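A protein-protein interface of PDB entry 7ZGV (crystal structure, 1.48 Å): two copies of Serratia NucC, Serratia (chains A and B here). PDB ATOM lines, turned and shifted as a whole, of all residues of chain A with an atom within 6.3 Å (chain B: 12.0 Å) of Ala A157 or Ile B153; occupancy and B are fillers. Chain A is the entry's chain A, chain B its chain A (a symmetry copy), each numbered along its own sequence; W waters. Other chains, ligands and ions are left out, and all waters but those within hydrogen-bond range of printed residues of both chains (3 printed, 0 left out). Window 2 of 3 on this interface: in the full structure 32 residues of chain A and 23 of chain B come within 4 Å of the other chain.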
ATOM      1  N   THR A 148      29.229   8.919  17.522  1.00  0.00           N
ATOM      2  CA  THR A 148      29.367  10.061  18.413  1.00  0.00           C
ATOM      3  C   THR A 148      28.129  10.260  19.268  1.00  0.00           C
ATOM      4  O   THR A 148      27.114   9.560  19.137  1.00  0.00           O
ATOM      5  CB  THR A 148      29.742  11.338  17.650  1.00  0.00           C
ATOM      6  OG1 THR A 148      28.713  11.692  16.717  1.00  0.00           O
ATOM      7  CG2 THR A 148      31.040  11.104  16.923  1.00  0.00           C
ATOM      8  N   VAL A 149      28.235  11.223  20.183  1.00  0.00           N
ATOM      9  CA  VAL A 149      27.146  11.470  21.117  1.00  0.00           C
ATOM     10  C   VAL A 149      25.920  11.948  20.351  1.00  0.00           C
ATOM     11  O   VAL A 149      26.014  12.513  19.249  1.00  0.00           O
ATOM     12  CB  VAL A 149      27.525  12.473  22.218  1.00  0.00           C
ATOM     13  CG1 VAL A 149      28.625  11.904  23.111  1.00  0.00           C
ATOM     14  CG2 VAL A 149      27.951  13.826  21.593  1.00  0.00           C
ATOM     15  N   ILE A 150      24.765  11.779  20.983  1.00  0.00           N
ATOM     16  CA  ILE A 150      23.471  12.006  20.347  1.00  0.00           C
ATOM     17  C   ILE A 150      22.605  12.955  21.173  1.00  0.00           C
ATOM     18  O   ILE A 150      22.050  12.570  22.215  1.00  0.00           O
ATOM     19  CB  ILE A 150      22.747  10.687  20.072  1.00  0.00           C
ATOM     20  CG1 ILE A 150      23.555   9.839  19.089  1.00  0.00           C
ATOM     21  CG2 ILE A 150      21.444  10.961  19.536  1.00  0.00           C
ATOM     22  CD1 ILE A 150      22.895   8.594  18.675  1.00  0.00           C
ATOM     23  N   LYS A 151      22.413  14.164  20.649  1.00  0.00           N
ATOM     24  CA  LYS A 151      21.497  15.114  21.252  1.00  0.00           C
ATOM     25  C   LYS A 151      20.064  14.701  20.978  1.00  0.00           C
ATOM     26  O   LYS A 151      19.699  14.378  19.842  1.00  0.00           O
ATOM     27  CB  LYS A 151      21.748  16.489  20.652  1.00  0.00           C
ATOM     28  CG  LYS A 151      20.927  17.593  21.283  1.00  0.00           C
ATOM     29  CD  LYS A 151      21.413  17.938  22.708  1.00  0.00           C
ATOM     30  CE  LYS A 151      20.407  18.822  23.424  1.00  0.00           C
ATOM     31  NZ  LYS A 151      19.148  18.052  23.761  1.00  0.00           N
ATOM     32  N   ASN A 152      19.255  14.702  22.022  1.00  0.00           N
ATOM     33  CA  ASN A 152      17.889  14.219  21.923  1.00  0.00           C
ATOM     34  C   ASN A 152      17.074  14.876  23.026  1.00  0.00           C
ATOM     35  O   ASN A 152      17.604  15.628  23.847  1.00  0.00           O
ATOM     36  CB  ASN A 152      17.853  12.680  21.957  1.00  0.00           C
ATOM     37  CG  ASN A 152      18.043  12.133  23.347  1.00  0.00           C
ATOM     38  OD1 ASN A 152      17.090  11.782  24.012  1.00  0.00           O
ATOM     39  ND2 ASN A 152      19.291  12.049  23.786  1.00  0.00           N
ATOM     40  N   GLY A 155      18.448  14.878  26.556  1.00  0.00           N
ATOM     41  CA  GLY A 155      19.749  15.450  26.832  1.00  0.00           C
ATOM     42  C   GLY A 155      20.726  15.065  25.746  1.00  0.00           C
ATOM     43  O   GLY A 155      20.486  15.364  24.568  1.00  0.00           O
ATOM     44  N   THR A 156      21.848  14.457  26.133  1.00  0.00           N
ATOM     45  CA  THR A 156      22.826  13.934  25.185  1.00  0.00           C
ATOM     46  C   THR A 156      23.153  12.512  25.597  1.00  0.00           C
ATOM     47  O   THR A 156      23.599  12.277  26.728  1.00  0.00           O
ATOM     48  CB  THR A 156      24.082  14.797  25.158  1.00  0.00           C
ATOM     49  OG1 THR A 156      23.742  16.110  24.699  1.00  0.00           O
ATOM     50  CG2 THR A 156      25.116  14.234  24.232  1.00  0.00           C
ATOM     51  N   ALA A 157      22.924  11.567  24.692  1.00  0.00           N
ATOM     52  CA  ALA A 157      23.217  10.163  24.966  1.00  0.00           C
ATOM     53  C   ALA A 157      24.651   9.838  24.580  1.00  0.00           C
ATOM     54  O   ALA A 157      25.203  10.409  23.640  1.00  0.00           O
ATOM     55  CB  ALA A 157      22.286   9.251  24.172  1.00  0.00           C
ATOM     56  N   LYS A 158      25.243   8.881  25.289  1.00  0.00           N
ATOM     57  CA  LYS A 158      26.568   8.422  24.893  1.00  0.00           C
ATOM     58  C   LYS A 158      26.499   7.749  23.522  1.00  0.00           C
ATOM     59  O   LYS A 158      25.416   7.335  23.068  1.00  0.00           O
ATOM     60  CB  LYS A 158      27.134   7.471  25.939  1.00  0.00           C
ATOM     61  CG  LYS A 158      26.514   6.119  25.990  1.00  0.00           C
ATOM     62  CD  LYS A 158      27.098   5.290  27.158  1.00  0.00           C
ATOM     63  CE  LYS A 158      26.790   3.796  27.020  1.00  0.00           C
ATOM     64  NZ  LYS A 158      25.343   3.494  26.797  1.00  0.00           N
ATOM     65  N   PRO A 159      27.641   7.631  22.836  1.00  0.00           N
ATOM     66  CA  PRO A 159      27.639   7.034  21.502  1.00  0.00           C
ATOM     67  C   PRO A 159      27.072   5.632  21.507  1.00  0.00           C
ATOM     68  O   PRO A 159      27.303   4.842  22.428  1.00  0.00           O
ATOM     69  CB  PRO A 159      29.122   7.028  21.111  1.00  0.00           C
ATOM     70  CG  PRO A 159      29.727   8.112  21.928  1.00  0.00           C
ATOM     71  CD  PRO A 159      29.001   8.034  23.238  1.00  0.00           C
ATOM     72  N   VAL A 160      26.325   5.341  20.445  1.00  0.00           N
ATOM     73  CA  VAL A 160      25.693   4.046  20.275  1.00  0.00           C
ATOM     74  C   VAL A 160      26.736   3.079  19.740  1.00  0.00           C
ATOM     75  O   VAL A 160      27.523   3.410  18.848  1.00  0.00           O
ATOM     76  CB  VAL A 160      24.492   4.183  19.326  1.00  0.00           C
ATOM     77  CG1 VAL A 160      23.900   2.849  19.048  1.00  0.00           C
ATOM     78  CG2 VAL A 160      23.441   5.129  19.936  1.00  0.00           C
ATOM     79  N   GLU A 161      26.735   1.875  20.293  1.00  0.00           N
ATOM     80  CA  GLU A 161      27.584   0.799  19.802  1.00  0.00           C
ATOM     81  C   GLU A 161      27.145   0.365  18.405  1.00  0.00           C
ATOM     82  O   GLU A 161      25.950   0.273  18.104  1.00  0.00           O
ATOM     83  CB  GLU A 161      27.490  -0.365  20.781  1.00  0.00           C
ATOM     84  CG  GLU A 161      27.381   0.080  22.269  1.00  0.00           C
ATOM     85  CD  GLU A 161      25.914   0.186  22.836  1.00  0.00           C
ATOM     86  OE1 GLU A 161      25.054   1.017  22.373  1.00  0.00           O
ATOM     87  OE2 GLU A 161      25.635  -0.577  23.795  1.00  0.00           O
ATOM     88  N   THR A 242      18.577   2.424  15.047  1.00  0.00           N
ATOM     89  CA  THR A 242      19.036   3.381  14.039  1.00  0.00           C
ATOM     90  C   THR A 242      20.567   3.404  14.008  1.00  0.00           C
ATOM     91  O   THR A 242      21.233   3.183  15.027  1.00  0.00           O
ATOM     92  CB  THR A 242      18.467   4.771  14.370  1.00  0.00           C
ATOM     93  OG1 THR A 242      17.032   4.699  14.274  1.00  0.00           O
ATOM     94  CG2 THR A 242      18.996   5.883  13.429  1.00  0.00           C
ATOM     95  N   TYR B  97       8.180   3.541  10.216  1.00  0.00           N
ATOM     96  CA  TYR B  97       8.599   2.366  10.970  1.00  0.00           C
ATOM     97  C   TYR B  97       7.882   1.106  10.570  1.00  0.00           C
ATOM     98  O   TYR B  97       8.353   0.028  10.917  1.00  0.00           O
ATOM     99  CB  TYR B  97       8.337   2.576  12.474  1.00  0.00           C
ATOM    100  CG  TYR B  97       9.169   3.702  13.024  1.00  0.00           C
ATOM    101  CD1 TYR B  97      10.519   3.504  13.259  1.00  0.00           C
ATOM    102  CD2 TYR B  97       8.627   4.954  13.307  1.00  0.00           C
ATOM    103  CE1 TYR B  97      11.319   4.525  13.737  1.00  0.00           C
ATOM    104  CE2 TYR B  97       9.419   5.978  13.809  1.00  0.00           C
ATOM    105  CZ  TYR B  97      10.757   5.745  14.018  1.00  0.00           C
ATOM    106  OH  TYR B  97      11.598   6.715  14.503  1.00  0.00           O
ATOM    107  N   VAL B 149       9.156  -4.768  21.723  1.00  0.00           N
ATOM    108  CA  VAL B 149      10.207  -3.953  22.317  1.00  0.00           C
ATOM    109  C   VAL B 149      10.838  -3.078  21.242  1.00  0.00           C
ATOM    110  O   VAL B 149      10.818  -3.396  20.042  1.00  0.00           O
ATOM    111  CB  VAL B 149      11.276  -4.795  23.030  1.00  0.00           C
ATOM    112  CG1 VAL B 149      10.678  -5.519  24.234  1.00  0.00           C
ATOM    113  CG2 VAL B 149      11.930  -5.792  22.040  1.00  0.00           C
ATOM    114  N   ILE B 150      11.465  -2.000  21.696  1.00  0.00           N
ATOM    115  CA  ILE B 150      11.974  -0.950  20.821  1.00  0.00           C
ATOM    116  C   ILE B 150      13.448  -0.661  21.101  1.00  0.00           C
ATOM    117  O   ILE B 150      13.795  -0.021  22.106  1.00  0.00           O
ATOM    118  CB  ILE B 150      11.129   0.321  20.923  1.00  0.00           C
ATOM    119  CG1 ILE B 150       9.701   0.040  20.455  1.00  0.00           C
ATOM    120  CG2 ILE B 150      11.719   1.354  20.122  1.00  0.00           C
ATOM    121  CD1 ILE B 150       8.831   1.223  20.413  1.00  0.00           C
ATOM    122  N   LYS B 151      14.301  -1.050  20.154  1.00  0.00           N
ATOM    123  CA  LYS B 151      15.710  -0.710  20.220  1.00  0.00           C
ATOM    124  C   LYS B 151      15.909   0.755  19.884  1.00  0.00           C
ATOM    125  O   LYS B 151      15.367   1.262  18.896  1.00  0.00           O
ATOM    126  CB  LYS B 151      16.468  -1.564  19.217  1.00  0.00           C
ATOM    127  CG  LYS B 151      17.972  -1.383  19.268  1.00  0.00           C
ATOM    128  CD  LYS B 151      18.591  -2.016  20.533  1.00  0.00           C
ATOM    129  CE  LYS B 151      20.031  -1.571  20.711  1.00  0.00           C
ATOM    130  NZ  LYS B 151      20.105  -0.107  21.094  1.00  0.00           N
ATOM    131  N   ASN B 152      16.680   1.435  20.713  1.00  0.00           N
ATOM    132  CA  ASN B 152      16.862   2.870  20.573  1.00  0.00           C
ATOM    133  C   ASN B 152      18.187   3.243  21.220  1.00  0.00           C
ATOM    134  O   ASN B 152      18.878   2.397  21.791  1.00  0.00           O
ATOM    135  CB  ASN B 152      15.653   3.629  21.150  1.00  0.00           C
ATOM    136  CG  ASN B 152      15.673   3.680  22.655  1.00  0.00           C
ATOM    137  OD1 ASN B 152      16.076   4.665  23.237  1.00  0.00           O
ATOM    138  ND2 ASN B 152      15.222   2.609  23.291  1.00  0.00           N
ATOM    139  N   ILE B 153      18.531   4.532  21.147  1.00  0.00           N
ATOM    140  CA  ILE B 153      19.840   4.979  21.631  1.00  0.00           C
ATOM    141  C   ILE B 153      20.073   4.627  23.098  1.00  0.00           C
ATOM    142  O   ILE B 153      21.223   4.511  23.534  1.00  0.00           O
ATOM    143  CB  ILE B 153      20.063   6.491  21.414  1.00  0.00           C
ATOM    144  CG1 ILE B 153      19.077   7.344  22.259  1.00  0.00           C
ATOM    145  CG2 ILE B 153      19.950   6.828  19.952  1.00  0.00           C
ATOM    146  CD1 ILE B 153      19.273   8.834  22.137  1.00  0.00           C
ATOM    147  N   TYR B 154      19.016   4.537  23.898  1.00  0.00           N
ATOM    148  CA  TYR B 154      19.184   4.280  25.325  1.00  0.00           C
ATOM    149  C   TYR B 154      19.073   2.800  25.681  1.00  0.00           C
ATOM    150  O   TYR B 154      19.168   2.443  26.865  1.00  0.00           O
ATOM    151  CB  TYR B 154      18.186   5.095  26.139  1.00  0.00           C
ATOM    152  CG  TYR B 154      18.505   6.569  26.185  1.00  0.00           C
ATOM    153  CD1 TYR B 154      19.644   7.024  26.827  1.00  0.00           C
ATOM    154  CD2 TYR B 154      17.667   7.496  25.596  1.00  0.00           C
ATOM    155  CE1 TYR B 154      19.953   8.376  26.873  1.00  0.00           C
ATOM    156  CE2 TYR B 154      17.965   8.863  25.650  1.00  0.00           C
ATOM    157  CZ  TYR B 154      19.115   9.283  26.292  1.00  0.00           C
ATOM    158  OH  TYR B 154      19.474  10.605  26.401  1.00  0.00           O
ATOM    159  N   GLY B 155      18.959   1.929  24.687  1.00  0.00           N
ATOM    160  CA  GLY B 155      18.949   0.505  24.947  1.00  0.00           C
ATOM    161  C   GLY B 155      17.776  -0.141  24.245  1.00  0.00           C
ATOM    162  O   GLY B 155      17.662  -0.036  23.016  1.00  0.00           O
ATOM    163  N   THR B 156      16.939  -0.852  25.000  1.00  0.00           N
ATOM    164  CA  THR B 156      15.710  -1.437  24.474  1.00  0.00           C
ATOM    165  C   THR B 156      14.582  -1.064  25.415  1.00  0.00           C
ATOM    166  O   THR B 156      14.638  -1.379  26.611  1.00  0.00           O
ATOM    167  CB  THR B 156      15.834  -2.952  24.343  1.00  0.00           C
ATOM    168  OG1 THR B 156      16.862  -3.259  23.396  1.00  0.00           O
ATOM    169  CG2 THR B 156      14.558  -3.566  23.861  1.00  0.00           C
ATOM    170  N   ALA B 157      13.569  -0.388  24.885  1.00  0.00           N
ATOM    171  CA  ALA B 157      12.416   0.010  25.688  1.00  0.00           C
ATOM    172  C   ALA B 157      11.364  -1.087  25.681  1.00  0.00           C
ATOM    173  O   ALA B 157      11.208  -1.815  24.701  1.00  0.00           O
ATOM    174  CB  ALA B 157      11.786   1.285  25.133  1.00  0.00           C
ATOM    175  N   LYS B 158      10.608  -1.175  26.772  1.00  0.00           N
ATOM    176  CA  LYS B 158       9.492  -2.112  26.787  1.00  0.00           C
ATOM    177  C   LYS B 158       8.443  -1.693  25.756  1.00  0.00           C
ATOM    178  O   LYS B 158       8.415  -0.531  25.312  1.00  0.00           O
ATOM    179  CB  LYS B 158       8.885  -2.192  28.181  1.00  0.00           C
ATOM    180  CG  LYS B 158       8.094  -1.007  28.612  1.00  0.00           C
ATOM    181  CD  LYS B 158       7.623  -1.162  30.077  1.00  0.00           C
ATOM    182  CE  LYS B 158       6.505  -0.180  30.436  1.00  0.00           C
ATOM    183  NZ  LYS B 158       6.819   1.243  30.105  1.00  0.00           N
HETATM  184  O   HOH W   1      21.131  11.254  28.223  1.00  0.00           O
HETATM  185  O   HOH W   2      23.074  -0.294  21.048  1.00  0.00           O
HETATM  186  O   HOH W   3      23.628   5.527  24.134  1.00  0.00           O
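Water W1 bridges the side-chain hydroxyl (OH) of Tyr B154 and the backbone carbonyl oxygen (O) of Thr A156.
Water W3 bridges the backbone carbonyl oxygen of Ile B153 (2.7 Å) and the backbone carbonyl oxygen of Lys A158 (2.8 Å).
Water W2 lies within hydrogen-bond range of the side-chain carboxylate of Glu A161 and the side-chain amino group of Lys B151.
Among the printed residues, pairs that only touch across the chains: Asn A152 with Ile B153 (3.6 Å), Ala A157 with Ile B153 (3.7 Å), Ile A150 with Ile B153 (3.7 Å), Ala A157 with Tyr B154 (3.7 Å) and Val A160 with Ile B153 (3.9 Å).
Hydrophobic or aromatic side chains of chain A that line the printed part of chain B: Ile A150, Ala A157 and Val A160.
Of the 11 printed residues of chain B, 2 touch a printed residue of chain A.
Hydrophobic or aromatic side chains of chain B that line the printed part of chain A: Ile B153 and Tyr B154.
Among the printed residues, 6 pairs touch across the chains.
Among the printed residues, no Asp or Glu carboxylate lies within 4 Å of a Lys or Arg side-chain nitrogen of the other chain.
The side-chain hydroxyl (OH) of Tyr B154 is in hydrogen-bond range of the side-chain amide nitrogen (ND2) of Asn A152, 3.0 Å away.
Of the printed residues of chain B, Ala A157 touches Ile B153 and Tyr B154.
Ile B153 touches just these residues of chain A: Ile A150, Asn A152, Ala A157 and Val A160.
No residue of chain B comes within 4 Å of Val A149.
No residue of chain B comes within 4 Å of Lys A151.
No residue of chain B comes within 4 Å of Thr A156.
No residue of chain B comes within 4 Å of Lys A158.
Printed residues of chain B within 4 Å of Val A160: Ile B153 (3.9 Å).
Of the printed residues of chain A, Tyr B154 touches Asn A152 and Ala A157.
Asn B152 touches none of the printed residues of chain A.
Thr B156 touches none of the printed residues of chain A.
The nearest residue of chain B that does not touch Ala A157 is Asn B152 (7.8 Å).
The nearest residue of chain A that does not touch Ile B153 is Lys A158 (5.1 Å).
O of Ile A150 sits at hydrogen-bond distance from ND2 of Asn A152, 3.2 Å away.
O of Ile A150 lies within hydrogen-bond range of N of Ala A157 (2.8 Å).
OD1 of Asn B152 lies within hydrogen-bond range of N of Tyr B154, at 3.0 Å.
8 positions are printed for both chains.
Of the 6 pairs that touch across the chains among the printed residues, none has its exchanged pair printed and touching as well.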
